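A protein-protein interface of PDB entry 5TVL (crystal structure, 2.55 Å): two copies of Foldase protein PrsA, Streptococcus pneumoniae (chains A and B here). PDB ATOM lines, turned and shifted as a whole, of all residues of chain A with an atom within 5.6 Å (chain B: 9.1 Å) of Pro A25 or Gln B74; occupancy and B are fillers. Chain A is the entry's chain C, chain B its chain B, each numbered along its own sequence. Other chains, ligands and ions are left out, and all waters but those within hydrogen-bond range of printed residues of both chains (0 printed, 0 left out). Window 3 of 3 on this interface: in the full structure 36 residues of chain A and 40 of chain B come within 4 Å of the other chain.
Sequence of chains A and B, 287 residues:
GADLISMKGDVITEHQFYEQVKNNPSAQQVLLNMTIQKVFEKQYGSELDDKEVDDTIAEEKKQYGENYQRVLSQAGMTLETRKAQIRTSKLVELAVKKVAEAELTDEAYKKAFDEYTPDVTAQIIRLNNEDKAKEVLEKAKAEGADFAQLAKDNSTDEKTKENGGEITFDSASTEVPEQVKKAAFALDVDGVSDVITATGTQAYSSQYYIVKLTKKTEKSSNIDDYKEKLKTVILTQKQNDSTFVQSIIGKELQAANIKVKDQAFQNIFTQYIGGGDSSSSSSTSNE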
ATOM      1  N   ASN A  23      35.139 -15.393  26.238  1.00  0.00           N
ATOM      2  CA  ASN A  23      33.669 -15.418  26.151  1.00  0.00           C
ATOM      3  C   ASN A  23      32.982 -14.281  26.920  1.00  0.00           C
ATOM      4  O   ASN A  23      31.792 -14.040  26.715  1.00  0.00           O
ATOM      5  CB  ASN A  23      33.136 -16.766  26.645  1.00  0.00           C
ATOM      6  CG  ASN A  23      33.686 -17.936  25.849  1.00  0.00           C
ATOM      7  OD1 ASN A  23      33.644 -17.936  24.615  1.00  0.00           O
ATOM      8  ND2 ASN A  23      34.217 -18.936  26.549  1.00  0.00           N
ATOM      9  N   ASN A  24      33.721 -13.602  27.798  1.00  0.00           N
ATOM     10  CA  ASN A  24      33.216 -12.446  28.545  1.00  0.00           C
ATOM     11  C   ASN A  24      32.863 -11.299  27.576  1.00  0.00           C
ATOM     12  O   ASN A  24      33.722 -10.884  26.797  1.00  0.00           O
ATOM     13  CB  ASN A  24      34.282 -11.982  29.556  1.00  0.00           C
ATOM     14  CG  ASN A  24      33.749 -10.987  30.572  1.00  0.00           C
ATOM     15  OD1 ASN A  24      33.539  -9.817  30.255  1.00  0.00           O
ATOM     16  ND2 ASN A  24      33.561 -11.438  31.808  1.00  0.00           N
ATOM     17  N   PRO A  25      31.612 -10.780  27.620  1.00  0.00           N
ATOM     18  CA  PRO A  25      31.236  -9.729  26.649  1.00  0.00           C
ATOM     19  C   PRO A  25      31.984  -8.402  26.820  1.00  0.00           C
ATOM     20  O   PRO A  25      32.162  -7.673  25.843  1.00  0.00           O
ATOM     21  CB  PRO A  25      29.727  -9.526  26.888  1.00  0.00           C
ATOM     22  CG  PRO A  25      29.306 -10.611  27.820  1.00  0.00           C
ATOM     23  CD  PRO A  25      30.527 -11.015  28.587  1.00  0.00           C
ATOM     24  N   SER A  26      32.402  -8.101  28.050  1.00  0.00           N
ATOM     25  CA  SER A  26      33.239  -6.932  28.337  1.00  0.00           C
ATOM     26  C   SER A  26      34.623  -7.086  27.685  1.00  0.00           C
ATOM     27  O   SER A  26      35.164  -6.127  27.130  1.00  0.00           O
ATOM     28  CB  SER A  26      33.371  -6.720  29.854  1.00  0.00           C
ATOM     29  OG  SER A  26      33.671  -5.379  30.171  1.00  0.00           O
ATOM     30  N   ALA A  27      35.177  -8.297  27.743  1.00  0.00           N
ATOM     31  CA  ALA A  27      36.438  -8.623  27.067  1.00  0.00           C
ATOM     32  C   ALA A  27      36.301  -8.654  25.543  1.00  0.00           C
ATOM     33  O   ALA A  27      37.243  -8.308  24.833  1.00  0.00           O
ATOM     34  CB  ALA A  27      36.970  -9.953  27.569  1.00  0.00           C
ATOM     35  N   GLN A  28      35.146  -9.081  25.038  1.00  0.00           N
ATOM     36  CA  GLN A  28      34.877  -9.054  23.590  1.00  0.00           C
ATOM     37  C   GLN A  28      34.807  -7.627  23.036  1.00  0.00           C
ATOM     38  O   GLN A  28      35.229  -7.375  21.901  1.00  0.00           O
ATOM     39  CB  GLN A  28      33.592  -9.816  23.243  1.00  0.00           C
ATOM     40  CG  GLN A  28      33.729 -11.327  23.391  1.00  0.00           C
ATOM     41  CD  GLN A  28      32.646 -12.118  22.677  1.00  0.00           C
ATOM     42  OE1 GLN A  28      31.794 -11.564  21.976  1.00  0.00           O
ATOM     43  NE2 GLN A  28      32.683 -13.434  22.847  1.00  0.00           N
ATOM     44  N   GLN A  29      34.274  -6.709  23.839  1.00  0.00           N
ATOM     45  CA  GLN A  29      34.238  -5.295  23.490  1.00  0.00           C
ATOM     46  C   GLN A  29      35.651  -4.727  23.373  1.00  0.00           C
ATOM     47  O   GLN A  29      35.908  -3.907  22.492  1.00  0.00           O
ATOM     48  CB  GLN A  29      33.417  -4.502  24.516  1.00  0.00           C
ATOM     49  CG  GLN A  29      33.044  -3.083  24.086  1.00  0.00           C
ATOM     50  CD  GLN A  29      32.114  -3.033  22.875  1.00  0.00           C
ATOM     51  OE1 GLN A  29      31.188  -3.842  22.750  1.00  0.00           O
ATOM     52  NE2 GLN A  29      32.349  -2.072  21.982  1.00  0.00           N
ATOM     53  N   VAL A  30      36.563  -5.175  24.241  1.00  0.00           N
ATOM     54  CA  VAL A  30      37.971  -4.734  24.199  1.00  0.00           C
ATOM     55  C   VAL A  30      38.660  -5.123  22.882  1.00  0.00           C
ATOM     56  O   VAL A  30      39.411  -4.325  22.324  1.00  0.00           O
ATOM     57  CB  VAL A  30      38.779  -5.252  25.420  1.00  0.00           C
ATOM     58  CG1 VAL A  30      40.275  -4.998  25.264  1.00  0.00           C
ATOM     59  CG2 VAL A  30      38.288  -4.588  26.695  1.00  0.00           C
ATOM     60  N   ILE A 268      30.280 -10.316  17.683  1.00  0.00           N
ATOM     61  CA  ILE A 268      30.446  -8.885  17.991  1.00  0.00           C
ATOM     62  C   ILE A 268      30.953  -8.039  16.798  1.00  0.00           C
ATOM     63  O   ILE A 268      30.724  -6.825  16.755  1.00  0.00           O
ATOM     64  CB  ILE A 268      31.344  -8.681  19.243  1.00  0.00           C
ATOM     65  CG1 ILE A 268      31.129  -7.285  19.845  1.00  0.00           C
ATOM     66  CG2 ILE A 268      32.815  -8.939  18.924  1.00  0.00           C
ATOM     67  CD1 ILE A 268      31.794  -7.077  21.187  1.00  0.00           C
ATOM     68  N   PHE B  17      46.138  -8.604  23.295  1.00  0.00           N
ATOM     69  CA  PHE B  17      44.791  -8.622  23.841  1.00  0.00           C
ATOM     70  C   PHE B  17      44.805  -8.820  25.359  1.00  0.00           C
ATOM     71  O   PHE B  17      44.059  -8.136  26.070  1.00  0.00           O
ATOM     72  CB  PHE B  17      43.936  -9.700  23.171  1.00  0.00           C
ATOM     73  CG  PHE B  17      42.593  -9.897  23.823  1.00  0.00           C
ATOM     74  CD1 PHE B  17      41.681  -8.852  23.878  1.00  0.00           C
ATOM     75  CD2 PHE B  17      42.246 -11.119  24.392  1.00  0.00           C
ATOM     76  CE1 PHE B  17      40.449  -9.019  24.474  1.00  0.00           C
ATOM     77  CE2 PHE B  17      41.007 -11.298  24.988  1.00  0.00           C
ATOM     78  CZ  PHE B  17      40.107 -10.244  25.031  1.00  0.00           C
ATOM     79  N   VAL B  21      43.181  -6.298  28.081  1.00  0.00           N
ATOM     80  CA  VAL B  21      42.036  -6.822  28.829  1.00  0.00           C
ATOM     81  C   VAL B  21      42.306  -7.051  30.326  1.00  0.00           C
ATOM     82  O   VAL B  21      41.360  -7.075  31.110  1.00  0.00           O
ATOM     83  CB  VAL B  21      41.478  -8.111  28.172  1.00  0.00           C
ATOM     84  CG1 VAL B  21      42.310  -9.337  28.533  1.00  0.00           C
ATOM     85  CG2 VAL B  21      40.015  -8.323  28.541  1.00  0.00           C
ATOM     86  N   ASN B  24      40.601  -4.638  32.628  1.00  0.00           N
ATOM     87  CA  ASN B  24      39.146  -4.641  32.587  1.00  0.00           C
ATOM     88  C   ASN B  24      38.610  -5.233  33.889  1.00  0.00           C
ATOM     89  O   ASN B  24      38.970  -6.357  34.230  1.00  0.00           O
ATOM     90  CB  ASN B  24      38.656  -5.464  31.394  1.00  0.00           C
ATOM     91  CG  ASN B  24      37.146  -5.457  31.255  1.00  0.00           C
ATOM     92  OD1 ASN B  24      36.460  -6.270  31.865  1.00  0.00           O
ATOM     93  ND2 ASN B  24      36.625  -4.554  30.435  1.00  0.00           N
ATOM     94  N   SER B  26      35.733  -6.532  34.816  1.00  0.00           N
ATOM     95  CA  SER B  26      34.989  -7.773  34.623  1.00  0.00           C
ATOM     96  C   SER B  26      35.932  -8.939  34.337  1.00  0.00           C
ATOM     97  O   SER B  26      35.678 -10.067  34.774  1.00  0.00           O
ATOM     98  CB  SER B  26      33.969  -7.618  33.495  1.00  0.00           C
ATOM     99  OG  SER B  26      33.047  -8.685  33.510  1.00  0.00           O
ATOM    100  N   ALA B  27      37.020  -8.656  33.618  1.00  0.00           N
ATOM    101  CA  ALA B  27      38.089  -9.636  33.401  1.00  0.00           C
ATOM    102  C   ALA B  27      38.834  -9.976  34.695  1.00  0.00           C
ATOM    103  O   ALA B  27      39.162 -11.137  34.924  1.00  0.00           O
ATOM    104  CB  ALA B  27      39.069  -9.139  32.348  1.00  0.00           C
ATOM    105  N   VAL B  30      37.090 -12.589  36.568  1.00  0.00           N
ATOM    106  CA  VAL B  30      37.242 -13.927  35.974  1.00  0.00           C
ATOM    107  C   VAL B  30      38.469 -14.649  36.533  1.00  0.00           C
ATOM    108  O   VAL B  30      38.368 -15.821  36.899  1.00  0.00           O
ATOM    109  CB  VAL B  30      37.287 -13.878  34.424  1.00  0.00           C
ATOM    110  CG1 VAL B  30      37.684 -15.224  33.826  1.00  0.00           C
ATOM    111  CG2 VAL B  30      35.934 -13.453  33.869  1.00  0.00           C
ATOM    112  N   ASN B  67      14.392 -18.799  28.573  1.00  0.00           N
ATOM    113  CA  ASN B  67      15.283 -17.633  28.625  1.00  0.00           C
ATOM    114  C   ASN B  67      16.715 -18.010  29.012  1.00  0.00           C
ATOM    115  O   ASN B  67      17.593 -17.149  29.002  1.00  0.00           O
ATOM    116  CB  ASN B  67      14.772 -16.601  29.640  1.00  0.00           C
ATOM    117  CG  ASN B  67      13.384 -16.075  29.307  1.00  0.00           C
ATOM    118  OD1 ASN B  67      13.106 -15.706  28.164  1.00  0.00           O
ATOM    119  ND2 ASN B  67      12.507 -16.023  30.308  1.00  0.00           N
ATOM    120  N   TYR B  68      16.960 -19.279  29.343  1.00  0.00           N
ATOM    121  CA  TYR B  68      18.227 -19.686  29.968  1.00  0.00           C
ATOM    122  C   TYR B  68      19.440 -19.481  29.051  1.00  0.00           C
ATOM    123  O   TYR B  68      20.442 -18.911  29.475  1.00  0.00           O
ATOM    124  CB  TYR B  68      18.143 -21.144  30.459  1.00  0.00           C
ATOM    125  CG  TYR B  68      19.192 -21.553  31.479  1.00  0.00           C
ATOM    126  CD1 TYR B  68      19.453 -20.766  32.603  1.00  0.00           C
ATOM    127  CD2 TYR B  68      19.895 -22.751  31.345  1.00  0.00           C
ATOM    128  CE1 TYR B  68      20.400 -21.148  33.545  1.00  0.00           C
ATOM    129  CE2 TYR B  68      20.843 -23.140  32.284  1.00  0.00           C
ATOM    130  CZ  TYR B  68      21.089 -22.335  33.382  1.00  0.00           C
ATOM    131  OH  TYR B  68      22.023 -22.708  34.318  1.00  0.00           O
ATOM    132  N   GLN B  69      19.336 -19.915  27.798  1.00  0.00           N
ATOM    133  CA  GLN B  69      20.411 -19.705  26.813  1.00  0.00           C
ATOM    134  C   GLN B  69      20.660 -18.215  26.545  1.00  0.00           C
ATOM    135  O   GLN B  69      21.806 -17.793  26.390  1.00  0.00           O
ATOM    136  CB  GLN B  69      20.097 -20.430  25.499  1.00  0.00           C
ATOM    137  CG  GLN B  69      21.259 -20.481  24.515  1.00  0.00           C
ATOM    138  CD  GLN B  69      21.008 -21.426  23.349  1.00  0.00           C
ATOM    139  OE1 GLN B  69      19.861 -21.690  22.977  1.00  0.00           O
ATOM    140  NE2 GLN B  69      22.085 -21.937  22.763  1.00  0.00           N
ATOM    141  N   ARG B  70      19.581 -17.436  26.498  1.00  0.00           N
ATOM    142  CA  ARG B  70      19.659 -15.985  26.316  1.00  0.00           C
ATOM    143  C   ARG B  70      20.319 -15.283  27.509  1.00  0.00           C
ATOM    144  O   ARG B  70      21.174 -14.416  27.318  1.00  0.00           O
ATOM    145  CB  ARG B  70      18.255 -15.426  26.067  1.00  0.00           C
ATOM    146  CG  ARG B  70      18.174 -13.922  25.841  1.00  0.00           C
ATOM    147  CD  ARG B  70      16.952 -13.559  25.009  1.00  0.00           C
ATOM    148  NE  ARG B  70      15.744 -14.271  25.444  1.00  0.00           N
ATOM    149  CZ  ARG B  70      14.621 -14.394  24.728  1.00  0.00           C
ATOM    150  NH1 ARG B  70      14.500 -13.845  23.515  1.00  0.00           N
ATOM    151  NH2 ARG B  70      13.595 -15.074  25.237  1.00  0.00           N
ATOM    152  N   VAL B  71      19.923 -15.669  28.724  1.00  0.00           N
ATOM    153  CA  VAL B  71      20.519 -15.145  29.968  1.00  0.00           C
ATOM    154  C   VAL B  71      21.984 -15.589  30.136  1.00  0.00           C
ATOM    155  O   VAL B  71      22.823 -14.807  30.595  1.00  0.00           O
ATOM    156  CB  VAL B  71      19.671 -15.544  31.210  1.00  0.00           C
ATOM    157  CG1 VAL B  71      20.390 -15.240  32.522  1.00  0.00           C
ATOM    158  CG2 VAL B  71      18.331 -14.822  31.186  1.00  0.00           C
ATOM    159  N   LEU B  72      22.279 -16.840  29.782  1.00  0.00           N
ATOM    160  CA  LEU B  72      23.658 -17.350  29.783  1.00  0.00           C
ATOM    161  C   LEU B  72      24.558 -16.585  28.809  1.00  0.00           C
ATOM    162  O   LEU B  72      25.700 -16.255  29.141  1.00  0.00           O
ATOM    163  CB  LEU B  72      23.693 -18.845  29.442  1.00  0.00           C
ATOM    164  CG  LEU B  72      23.275 -19.843  30.524  1.00  0.00           C
ATOM    165  CD1 LEU B  72      23.093 -21.225  29.914  1.00  0.00           C
ATOM    166  CD2 LEU B  72      24.288 -19.890  31.659  1.00  0.00           C
ATOM    167  N   SER B  73      24.043 -16.311  27.612  1.00  0.00           N
ATOM    168  CA  SER B  73      24.795 -15.551  26.597  1.00  0.00           C
ATOM    169  C   SER B  73      25.072 -14.111  27.037  1.00  0.00           C
ATOM    170  O   SER B  73      26.145 -13.584  26.756  1.00  0.00           O
ATOM    171  CB  SER B  73      24.072 -15.559  25.246  1.00  0.00           C
ATOM    172  OG  SER B  73      24.074 -16.856  24.674  1.00  0.00           O
ATOM    173  N   GLN B  74      24.115 -13.497  27.735  1.00  0.00           N
ATOM    174  CA  GLN B  74      24.300 -12.170  28.346  1.00  0.00           C
ATOM    175  C   GLN B  74      25.488 -12.154  29.324  1.00  0.00           C
ATOM    176  O   GLN B  74      26.262 -11.196  29.351  1.00  0.00           O
ATOM    177  CB  GLN B  74      23.008 -11.737  29.064  1.00  0.00           C
ATOM    178  CG  GLN B  74      23.006 -10.327  29.646  1.00  0.00           C
ATOM    179  CD  GLN B  74      22.885  -9.232  28.602  1.00  0.00           C
ATOM    180  OE1 GLN B  74      22.766  -9.498  27.406  1.00  0.00           O
ATOM    181  NE2 GLN B  74      22.902  -7.984  29.056  1.00  0.00           N
ATOM    182  N   ALA B  75      25.622 -13.218  30.114  1.00  0.00           N
ATOM    183  CA  ALA B  75      26.728 -13.362  31.066  1.00  0.00           C
ATOM    184  C   ALA B  75      28.049 -13.817  30.422  1.00  0.00           C
ATOM    185  O   ALA B  75      29.094 -13.782  31.077  1.00  0.00           O
ATOM    186  CB  ALA B  75      26.333 -14.325  32.175  1.00  0.00           C
ATOM    187  N   GLY B  76      28.002 -14.255  29.163  1.00  0.00           N
ATOM    188  CA  GLY B  76      29.188 -14.715  28.445  1.00  0.00           C
ATOM    189  C   GLY B  76      29.551 -16.109  28.899  1.00  0.00           C
ATOM    190  O   GLY B  76      30.693 -16.372  29.292  1.00  0.00           O
ATOM    191  N   MET B  77      28.564 -16.999  28.852  1.00  0.00           N
ATOM    192  CA  MET B  77      28.693 -18.346  29.394  1.00  0.00           C
ATOM    193  C   MET B  77      27.861 -19.352  28.616  1.00  0.00           C
ATOM    194  O   MET B  77      26.934 -18.987  27.881  1.00  0.00           O
ATOM    195  CB  MET B  77      28.256 -18.359  30.861  1.00  0.00           C
ATOM    196  CG  MET B  77      29.255 -17.720  31.807  1.00  0.00           C
ATOM    197  SD  MET B  77      28.886 -18.118  33.518  1.00  0.00           S
ATOM    198  CE  MET B  77      27.487 -17.050  33.845  1.00  0.00           C
ATOM    199  N   THR B  78      28.213 -20.623  28.797  1.00  0.00           N
ATOM    200  CA  THR B  78      27.450 -21.749  28.259  1.00  0.00           C
ATOM    201  C   THR B  78      27.009 -22.652  29.418  1.00  0.00           C
ATOM    202  O   THR B  78      27.326 -22.381  30.581  1.00  0.00           O
ATOM    203  CB  THR B  78      28.243 -22.520  27.172  1.00  0.00           C
ATOM    204  OG1 THR B  78      27.389 -23.491  26.552  1.00  0.00           O
ATOM    205  CG2 THR B  78      29.488 -23.218  27.734  1.00  0.00           C
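The side-chain amide nitrogen (ND2) of Asn B24 lies within hydrogen-bond range of the side-chain hydroxyl (OG) of Ser A26 (3.1 Å).
ND2 of Asn A24 lies within hydrogen-bond range of OG of Ser B26 (3.3 Å).
Asn A24 touches Ser B26, and with the chains exchanged Ser A26 touches Asn B24.
Asn A24 touches Val B30, but with the chains exchanged Val A30 does not touch Asn B24 (4.1 Å).
Ser A26 touches its own counterpart, Ser B26.
Positions printed for both chains: 24, 26, 27 and 30.
Of the printed residues of chain B, Pro A25 touches Gln B74 (3.5 Å), Ala B75 (3.99 Å) and Gly B76 (3.9 Å).
Gln B74 touches just one residue of chain A: Pro A25 (3.5 Å).
Asn A24 touches just these residues of chain B: Ser B26 (3.3 Å) and Val B30 (3.7 Å).
Ser A26 touches just these residues of chain B: Asn B24 and Ser B26.
Printed residues of chain A within 4 Å of Val B21: Ala A27.
Printed residues of chain A within 4 Å of Asn B24: Ser A26 (3.1 Å).
Of the printed residues of chain B, Ala A27 touches Phe B17 and Val B21.
Of the printed residues of chain A, Ser B26 touches Asn A24 and Ser A26.
Asn B67 touches none of the printed residues of chain A.
Thr B78 touches none of the printed residues of chain A.
The nearest printed residue of chain A that does not touch Gln B74 is Asn A23 (6.8 Å).
Hydrophobic or aromatic side chains of chain B that line the printed part of chain A: Phe B17, Val B21 and Val B30.
Along chain B the printed residues that touch a printed residue of chain A span positions 17 to 76.
Among the printed residues, 10 pairs touch across the chains.
CA of Gly B76 touches O of Asn A23, 3.2 Å away.
ND2 of Asn A24 touches CG2 of Val B30 (3.7 Å).
O of Gln B74 touches CG of Pro A25, 3.5 Å away.
Pro A25 touches Ala B75.
Pro A25 touches Gly B76 (CD to CA, 3.9 Å).
Ser A26 touches Ser B26 (CB to CB, 3.8 Å).
O of Ala A27 touches CE1 of Phe B17, 3.3 Å away.
Ala A27 touches Val B21 (CB to CG2, 3.6 Å).
N of Ser B26 lies within hydrogen-bond range of OD1 of Asn B24.
The side-chain amide oxygen (OD1) of Asn B24 lies within hydrogen-bond range of the backbone NH (N) of Ala B27, 3.0 Å away.
The backbone NH (N) of Ser A26 is in hydrogen-bond range of the side-chain amide oxygen (OD1) of Asn A24 (3.0 Å).
The side-chain amide oxygen of Asn A24 lies within hydrogen-bond range of the backbone NH of Ala A27 (3.4 Å).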
